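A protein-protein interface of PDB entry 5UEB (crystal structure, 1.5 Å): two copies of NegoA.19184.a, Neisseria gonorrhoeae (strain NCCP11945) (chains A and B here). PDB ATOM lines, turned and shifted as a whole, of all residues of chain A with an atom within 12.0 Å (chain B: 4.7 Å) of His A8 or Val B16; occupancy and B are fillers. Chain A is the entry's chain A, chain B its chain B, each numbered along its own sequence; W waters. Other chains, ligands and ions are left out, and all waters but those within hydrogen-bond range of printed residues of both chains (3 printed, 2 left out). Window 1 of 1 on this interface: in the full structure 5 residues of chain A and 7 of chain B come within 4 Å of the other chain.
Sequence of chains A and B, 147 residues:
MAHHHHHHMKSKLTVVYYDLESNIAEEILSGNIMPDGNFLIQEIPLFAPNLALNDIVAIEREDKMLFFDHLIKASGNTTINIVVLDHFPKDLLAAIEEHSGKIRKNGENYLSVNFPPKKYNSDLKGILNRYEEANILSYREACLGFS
ND1 of His A7 is in hydrogen-bond range of OE2 of Glu B26 (2.7 Å).
NE2 of His A8 is in hydrogen-bond range of OE1 of Glu B60, at 3.4 Å.
A ring nitrogen (ND1) of His A8 sits at hydrogen-bond distance from the side-chain carboxylate (OE1) of Glu B62 (2.8 Å).
NZ of Lys A10 is in salt-bridge range of OE2 of Glu B60, 2.9 Å away.
The side-chain amide oxygen of Asn A32 sits close to the side-chain carboxylate of Glu B60 (3.0 Å).
NZ of Lys A10 is in hydrogen-bond range of OD1 of Asn A32 (2.7 Å).
NZ of Lys A10 lies within hydrogen-bond range of OE1 of Gln A42 (2.8 Å).
ND2 of Asn A32 is in hydrogen-bond range of OE1 of Gln A42, at 3.3 Å.
O of Glu B60 is in hydrogen-bond range of N of Phe B67, at 2.8 Å.
Among the printed residues, pairs that only touch across the chains: His A7 with Ile B24, His A8 with Phe B67, Met A9 with Ile B24 and His A8 with Val B16.
Printed residues of chain B within 4 Å of His A8: Val B16, Glu B60, Glu B62 and Phe B67.
Val B16 touches just one residue of chain A: His A8 (3.96 Å).
No residue of chain A comes within 4 Å of Val B15.
No residue of chain A comes within 4 Å of Tyr B17.
Printed residues of chain A within 4 Å of Ile B24: His A7 (3.3 Å) and Met A9 (3.6 Å).
No residue of chain A comes within 4 Å of Ala B25.
Of chain A, only His A7 comes within 4 Å of Glu B26.
Of chain A, only His A8 (3.5 Å) comes within 4 Å of Phe B67.
Of the printed residues of chain B, Asn A32 touches Glu B60 (3.0 Å).
Of the printed residues of chain A, Glu B62 touches His A8.
Printed residues of chain B within 4 Å of Lys A10: Glu B60 (2.9 Å).
Printed residues of chain B within 4 Å of Met A9: Ile B24 (3.6 Å).
Of the printed residues of chain B, His A7 touches Ile B24 and Glu B26.
The nearest printed residue of chain B that does not touch His A8 is Glu B26 (4.8 Å).
The nearest residue of chain A that does not touch Val B16 is His A7 (4.6 Å).
The nearest printed residue of chain B that does not touch His A7 is Val B16 (4.6 Å).
Printed residues of chain A that touch a printed residue of chain B: His A7, His A8, Met A9, Lys A10 and Asn A32.
Hydrophobic or aromatic side chains of chain A that line the printed part of chain B: His A7, His A8 and Met A9.
Among the printed residues, 9 pairs touch across the chains.
Among the printed residues, Asp or Glu carboxylates within 4 Å of a Lys or Arg side-chain nitrogen of the other chain: Lys A10 with Glu B60 (2.9 Å).
No position is printed for both chains.
Water W3 bridges the side-chain carboxylate (OE2) of Glu B60 (2.5 Å) and the side-chain amide nitrogen (ND2) of Asn A32 (3.3 Å).
Water W1 bridges the side-chain carboxylate (OE2) of Glu B62 (2.8 Å) and the backbone NH (N) of Met A9 (2.9 Å).
Water W2 lies within hydrogen-bond range of a ring nitrogen (NE2) of His A8 (2.8 Å) and the side-chain carboxylate (OE1) of Glu B60 (3.2 Å).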
ATOM      1  N   HIS A   6      -9.359 -21.940  -5.915  1.00  0.00           N
ATOM      2  CA  HIS A   6      -8.604 -22.144  -7.145  1.00  0.00           C
ATOM      3  C   HIS A   6      -7.236 -21.475  -7.063  1.00  0.00           C
ATOM      4  O   HIS A   6      -7.135 -20.250  -7.009  1.00  0.00           O
ATOM      5  CB  HIS A   6      -9.380 -21.596  -8.346  1.00  0.00           C
ATOM      6  N   HIS A   7      -6.184 -22.289  -7.041  1.00  0.00           N
ATOM      7  CA  HIS A   7      -4.814 -21.802  -7.027  1.00  0.00           C
ATOM      8  C   HIS A   7      -4.028 -22.526  -8.111  1.00  0.00           C
ATOM      9  O   HIS A   7      -4.375 -23.639  -8.513  1.00  0.00           O
ATOM     10  CB  HIS A   7      -4.139 -22.041  -5.665  1.00  0.00           C
ATOM     11  CG  HIS A   7      -4.746 -21.262  -4.537  1.00  0.00           C
ATOM     12  ND1 HIS A   7      -4.285 -20.020  -4.156  1.00  0.00           N
ATOM     13  CD2 HIS A   7      -5.771 -21.555  -3.701  1.00  0.00           C
ATOM     14  CE1 HIS A   7      -5.004 -19.579  -3.138  1.00  0.00           C
ATOM     15  NE2 HIS A   7      -5.912 -20.491  -2.844  1.00  0.00           N
ATOM     16  N   HIS A   8      -2.964 -21.881  -8.587  1.00  0.00           N
ATOM     17  CA  HIS A   8      -2.109 -22.516  -9.582  1.00  0.00           C
ATOM     18  C   HIS A   8      -1.476 -23.771  -8.998  1.00  0.00           C
ATOM     19  O   HIS A   8      -0.947 -23.750  -7.882  1.00  0.00           O
ATOM     20  CB  HIS A   8      -1.019 -21.555 -10.038  1.00  0.00           C
ATOM     21  CG  HIS A   8       0.021 -22.193 -10.905  1.00  0.00           C
ATOM     22  ND1 HIS A   8      -0.194 -22.481 -12.237  1.00  0.00           N
ATOM     23  CD2 HIS A   8       1.283 -22.601 -10.631  1.00  0.00           C
ATOM     24  CE1 HIS A   8       0.892 -23.035 -12.744  1.00  0.00           C
ATOM     25  NE2 HIS A   8       1.803 -23.118 -11.791  1.00  0.00           N
ATOM     26  N   MET A   9      -1.535 -24.863  -9.762  1.00  0.00           N
ATOM     27  CA  MET A   9      -1.079 -26.174  -9.328  1.00  0.00           C
ATOM     28  C   MET A   9      -0.374 -26.865 -10.484  1.00  0.00           C
ATOM     29  O   MET A   9      -0.619 -26.566 -11.654  1.00  0.00           O
ATOM     30  CB  MET A   9      -2.264 -27.059  -8.917  1.00  0.00           C
ATOM     31  CG  MET A   9      -2.911 -26.675  -7.606  1.00  0.00           C
ATOM     32  SD  MET A   9      -1.832 -26.992  -6.199  1.00  0.00           S
ATOM     33  CE  MET A   9      -2.549 -25.888  -4.982  1.00  0.00           C
ATOM     34  N   LYS A  10       0.516 -27.789 -10.144  1.00  0.00           N
ATOM     35  CA  LYS A  10       1.035 -28.729 -11.128  1.00  0.00           C
ATOM     36  C   LYS A  10      -0.079 -29.663 -11.587  1.00  0.00           C
ATOM     37  O   LYS A  10      -1.012 -29.963 -10.838  1.00  0.00           O
ATOM     38  CB  LYS A  10       2.135 -29.588 -10.496  1.00  0.00           C
ATOM     39  CG  LYS A  10       3.482 -28.911 -10.408  1.00  0.00           C
ATOM     40  CD  LYS A  10       4.041 -28.731 -11.800  1.00  0.00           C
ATOM     41  CE  LYS A  10       5.443 -28.187 -11.771  1.00  0.00           C
ATOM     42  NZ  LYS A  10       5.869 -27.853 -13.153  1.00  0.00           N
ATOM     43  N   SER A  11       0.024 -30.128 -12.833  1.00  0.00           N
ATOM     44  CA  SER A  11      -0.837 -31.221 -13.251  1.00  0.00           C
ATOM     45  C   SER A  11      -0.482 -32.491 -12.488  1.00  0.00           C
ATOM     46  O   SER A  11       0.623 -32.645 -11.952  1.00  0.00           O
ATOM     47  CB  SER A  11      -0.735 -31.457 -14.755  1.00  0.00           C
ATOM     48  OG  SER A  11      -1.330 -30.378 -15.453  1.00  0.00           O
ATOM     49  N   LYS A  12      -1.441 -33.408 -12.434  1.00  0.00           N
ATOM     50  CA  LYS A  12      -1.321 -34.602 -11.610  1.00  0.00           C
ATOM     51  C   LYS A  12      -1.616 -35.838 -12.444  1.00  0.00           C
ATOM     52  O   LYS A  12      -2.640 -35.903 -13.133  1.00  0.00           O
ATOM     53  CB  LYS A  12      -2.303 -34.537 -10.441  1.00  0.00           C
ATOM     54  CG  LYS A  12      -2.176 -33.275  -9.618  1.00  0.00           C
ATOM     55  CD  LYS A  12      -0.894 -33.268  -8.823  1.00  0.00           C
ATOM     56  CE  LYS A  12      -0.747 -31.959  -8.061  1.00  0.00           C
ATOM     57  NZ  LYS A  12       0.336 -32.013  -7.039  1.00  0.00           N
ATOM     58  N   SER A  30       3.103 -35.415  -9.447  1.00  0.00           N
ATOM     59  CA  SER A  30       3.049 -34.081 -10.029  1.00  0.00           C
ATOM     60  C   SER A  30       3.930 -34.000 -11.271  1.00  0.00           C
ATOM     61  O   SER A  30       4.940 -34.702 -11.393  1.00  0.00           O
ATOM     62  CB  SER A  30       3.536 -33.041  -9.020  1.00  0.00           C
ATOM     63  OG  SER A  30       2.668 -32.964  -7.902  1.00  0.00           O
ATOM     64  N   GLY A  31       3.549 -33.116 -12.190  1.00  0.00           N
ATOM     65  CA  GLY A  31       4.322 -32.927 -13.404  1.00  0.00           C
ATOM     66  C   GLY A  31       3.609 -31.987 -14.356  1.00  0.00           C
ATOM     67  O   GLY A  31       2.700 -31.256 -13.957  1.00  0.00           O
ATOM     68  N   ASN A  32       4.021 -32.031 -15.621  1.00  0.00           N
ATOM     69  CA  ASN A  32       3.566 -31.082 -16.631  1.00  0.00           C
ATOM     70  C   ASN A  32       2.954 -31.809 -17.814  1.00  0.00           C
ATOM     71  O   ASN A  32       3.493 -32.814 -18.284  1.00  0.00           O
ATOM     72  CB  ASN A  32       4.731 -30.281 -17.197  1.00  0.00           C
ATOM     73  CG  ASN A  32       5.254 -29.264 -16.228  1.00  0.00           C
ATOM     74  OD1 ASN A  32       4.531 -28.808 -15.343  1.00  0.00           O
ATOM     75  ND2 ASN A  32       6.516 -28.891 -16.387  1.00  0.00           N
ATOM     76  N   ILE A  33       1.846 -31.269 -18.315  1.00  0.00           N
ATOM     77  CA  ILE A  33       1.320 -31.671 -19.614  1.00  0.00           C
ATOM     78  C   ILE A  33       2.115 -30.910 -20.667  1.00  0.00           C
ATOM     79  O   ILE A  33       2.109 -29.672 -20.694  1.00  0.00           O
ATOM     80  CB  ILE A  33      -0.183 -31.371 -19.722  1.00  0.00           C
ATOM     81  CG1 ILE A  33      -0.965 -32.118 -18.641  1.00  0.00           C
ATOM     82  CG2 ILE A  33      -0.714 -31.770 -21.089  1.00  0.00           C
ATOM     83  CD1 ILE A  33      -2.448 -31.781 -18.629  1.00  0.00           C
ATOM     84  N   GLN A  42       7.530 -35.176 -12.636  1.00  0.00           N
ATOM     85  CA  GLN A  42       8.435 -34.256 -11.943  1.00  0.00           C
ATOM     86  C   GLN A  42       8.578 -34.555 -10.453  1.00  0.00           C
ATOM     87  O   GLN A  42       9.048 -33.700  -9.690  1.00  0.00           O
ATOM     88  CB  GLN A  42       8.043 -32.800 -12.196  1.00  0.00           C
ATOM     89  CG  GLN A  42       8.195 -32.417 -13.653  1.00  0.00           C
ATOM     90  CD  GLN A  42       7.945 -30.950 -13.898  1.00  0.00           C
ATOM     91  OE1 GLN A  42       6.887 -30.428 -13.546  1.00  0.00           O
ATOM     92  NE2 GLN A  42       8.927 -30.268 -14.489  1.00  0.00           N
ATOM     93  N   THR B  14       4.225 -14.868  -9.025  1.00  0.00           N
ATOM     94  CA  THR B  14       3.478 -15.387  -7.877  1.00  0.00           C
ATOM     95  C   THR B  14       4.092 -16.707  -7.414  1.00  0.00           C
ATOM     96  O   THR B  14       4.300 -17.615  -8.217  1.00  0.00           O
ATOM     97  CB  THR B  14       2.004 -15.594  -8.229  1.00  0.00           C
ATOM     98  OG1 THR B  14       1.419 -14.331  -8.563  1.00  0.00           O
ATOM     99  CG2 THR B  14       1.241 -16.211  -7.045  1.00  0.00           C
ATOM    100  N   VAL B  15       4.405 -16.796  -6.120  1.00  0.00           N
ATOM    101  CA  VAL B  15       4.863 -18.032  -5.496  1.00  0.00           C
ATOM    102  C   VAL B  15       3.695 -18.610  -4.711  1.00  0.00           C
ATOM    103  O   VAL B  15       3.207 -17.979  -3.766  1.00  0.00           O
ATOM    104  CB  VAL B  15       6.054 -17.780  -4.556  1.00  0.00           C
ATOM    105  CG1 VAL B  15       6.559 -19.105  -3.966  1.00  0.00           C
ATOM    106  CG2 VAL B  15       7.169 -17.073  -5.281  1.00  0.00           C
ATOM    107  N   VAL B  16       3.238 -19.799  -5.098  1.00  0.00           N
ATOM    108  CA  VAL B  16       2.229 -20.530  -4.336  1.00  0.00           C
ATOM    109  C   VAL B  16       2.956 -21.408  -3.327  1.00  0.00           C
ATOM    110  O   VAL B  16       3.931 -22.091  -3.672  1.00  0.00           O
ATOM    111  CB  VAL B  16       1.339 -21.373  -5.264  1.00  0.00           C
ATOM    112  CG1 VAL B  16       0.283 -22.125  -4.459  1.00  0.00           C
ATOM    113  CG2 VAL B  16       0.662 -20.495  -6.301  1.00  0.00           C
ATOM    114  N   TYR B  17       2.524 -21.352  -2.068  1.00  0.00           N
ATOM    115  CA  TYR B  17       3.211 -22.082  -1.008  1.00  0.00           C
ATOM    116  C   TYR B  17       2.195 -22.450   0.064  1.00  0.00           C
ATOM    117  O   TYR B  17       1.067 -21.954   0.075  1.00  0.00           O
ATOM    118  CB  TYR B  17       4.375 -21.252  -0.418  1.00  0.00           C
ATOM    119  CG  TYR B  17       3.922 -19.995   0.291  1.00  0.00           C
ATOM    120  CD1 TYR B  17       3.577 -18.849  -0.419  1.00  0.00           C
ATOM    121  CD2 TYR B  17       3.829 -19.955   1.677  1.00  0.00           C
ATOM    122  CE1 TYR B  17       3.127 -17.710   0.226  1.00  0.00           C
ATOM    123  CE2 TYR B  17       3.388 -18.807   2.341  1.00  0.00           C
ATOM    124  CZ  TYR B  17       3.043 -17.686   1.604  1.00  0.00           C
ATOM    125  OH  TYR B  17       2.590 -16.561   2.256  1.00  0.00           O
ATOM    126  N   ILE B  24      -2.917 -23.120   1.919  1.00  0.00           N
ATOM    127  CA  ILE B  24      -2.366 -22.592   0.683  1.00  0.00           C
ATOM    128  C   ILE B  24      -2.344 -21.070   0.746  1.00  0.00           C
ATOM    129  O   ILE B  24      -3.241 -20.434   1.317  1.00  0.00           O
ATOM    130  CB  ILE B  24      -3.175 -23.132  -0.511  1.00  0.00           C
ATOM    131  CG1 ILE B  24      -2.395 -22.948  -1.808  1.00  0.00           C
ATOM    132  CG2 ILE B  24      -4.555 -22.498  -0.568  1.00  0.00           C
ATOM    133  CD1 ILE B  24      -1.403 -24.064  -2.042  1.00  0.00           C
ATOM    134  N   ALA B  25      -1.289 -20.482   0.189  1.00  0.00           N
ATOM    135  CA  ALA B  25      -1.080 -19.042   0.223  1.00  0.00           C
ATOM    136  C   ALA B  25      -0.301 -18.641  -1.021  1.00  0.00           C
ATOM    137  O   ALA B  25       0.268 -19.484  -1.717  1.00  0.00           O
ATOM    138  CB  ALA B  25      -0.329 -18.614   1.490  1.00  0.00           C
ATOM    139  N   GLU B  26      -0.286 -17.338  -1.303  1.00  0.00           N
ATOM    140  CA  GLU B  26       0.415 -16.810  -2.465  1.00  0.00           C
ATOM    141  C   GLU B  26       1.184 -15.565  -2.054  1.00  0.00           C
ATOM    142  O   GLU B  26       0.668 -14.739  -1.296  1.00  0.00           O
ATOM    143  CB  GLU B  26      -0.581 -16.444  -3.577  1.00  0.00           C
ATOM    144  CG  GLU B  26      -1.311 -17.646  -4.140  1.00  0.00           C
ATOM    145  CD  GLU B  26      -2.270 -17.292  -5.256  1.00  0.00           C
ATOM    146  OE1 GLU B  26      -2.206 -16.151  -5.762  1.00  0.00           O
ATOM    147  OE2 GLU B  26      -3.092 -18.158  -5.621  1.00  0.00           O
ATOM    148  N   GLU B  60       6.420 -20.483 -14.889  1.00  0.00           N
ATOM    149  CA  GLU B  60       5.385 -21.028 -15.758  1.00  0.00           C
ATOM    150  C   GLU B  60       4.301 -19.980 -15.928  1.00  0.00           C
ATOM    151  O   GLU B  60       3.955 -19.281 -14.973  1.00  0.00           O
ATOM    152  CB  GLU B  60       4.715 -22.251 -15.136  1.00  0.00           C
ATOM    153  CG  GLU B  60       5.539 -23.505 -15.137  1.00  0.00           C
ATOM    154  CD  GLU B  60       4.704 -24.736 -14.806  1.00  0.00           C
ATOM    155  OE1 GLU B  60       3.619 -24.580 -14.204  1.00  0.00           O
ATOM    156  OE2 GLU B  60       5.127 -25.856 -15.153  1.00  0.00           O
ATOM    157  N   GLU B  62       0.363 -19.181 -16.619  1.00  0.00           N
ATOM    158  CA  GLU B  62      -0.990 -19.712 -16.569  1.00  0.00           C
ATOM    159  C   GLU B  62      -1.950 -18.548 -16.372  1.00  0.00           C
ATOM    160  O   GLU B  62      -1.661 -17.640 -15.588  1.00  0.00           O
ATOM    161  CB  GLU B  62      -1.140 -20.701 -15.406  1.00  0.00           C
ATOM    162  CG  GLU B  62      -2.465 -21.442 -15.375  1.00  0.00           C
ATOM    163  CD  GLU B  62      -2.578 -22.361 -14.175  1.00  0.00           C
ATOM    164  OE1 GLU B  62      -2.750 -21.851 -13.045  1.00  0.00           O
ATOM    165  OE2 GLU B  62      -2.471 -23.591 -14.359  1.00  0.00           O
ATOM    166  N   PHE B  67       4.151 -17.710 -12.654  1.00  0.00           N
ATOM    167  CA  PHE B  67       4.233 -18.432 -11.385  1.00  0.00           C
ATOM    168  C   PHE B  67       5.603 -19.060 -11.199  1.00  0.00           C
ATOM    169  O   PHE B  67       6.204 -19.557 -12.149  1.00  0.00           O
ATOM    170  CB  PHE B  67       3.169 -19.531 -11.298  1.00  0.00           C
ATOM    171  CG  PHE B  67       1.781 -18.999 -11.291  1.00  0.00           C
ATOM    172  CD1 PHE B  67       1.093 -18.800 -12.481  1.00  0.00           C
ATOM    173  CD2 PHE B  67       1.171 -18.671 -10.093  1.00  0.00           C
ATOM    174  CE1 PHE B  67      -0.196 -18.292 -12.471  1.00  0.00           C
ATOM    175  CE2 PHE B  67      -0.111 -18.163 -10.071  1.00  0.00           C
ATOM    176  CZ  PHE B  67      -0.794 -17.970 -11.268  1.00  0.00           C
HETATM  177  O   HOH W   1      -3.403 -24.655 -11.936  1.00  0.00           O
HETATM  178  O   HOH W   2       4.435 -23.938 -11.223  1.00  0.00           O
HETATM  179  O   HOH W   3       7.217 -25.669 -16.552  1.00  0.00           O
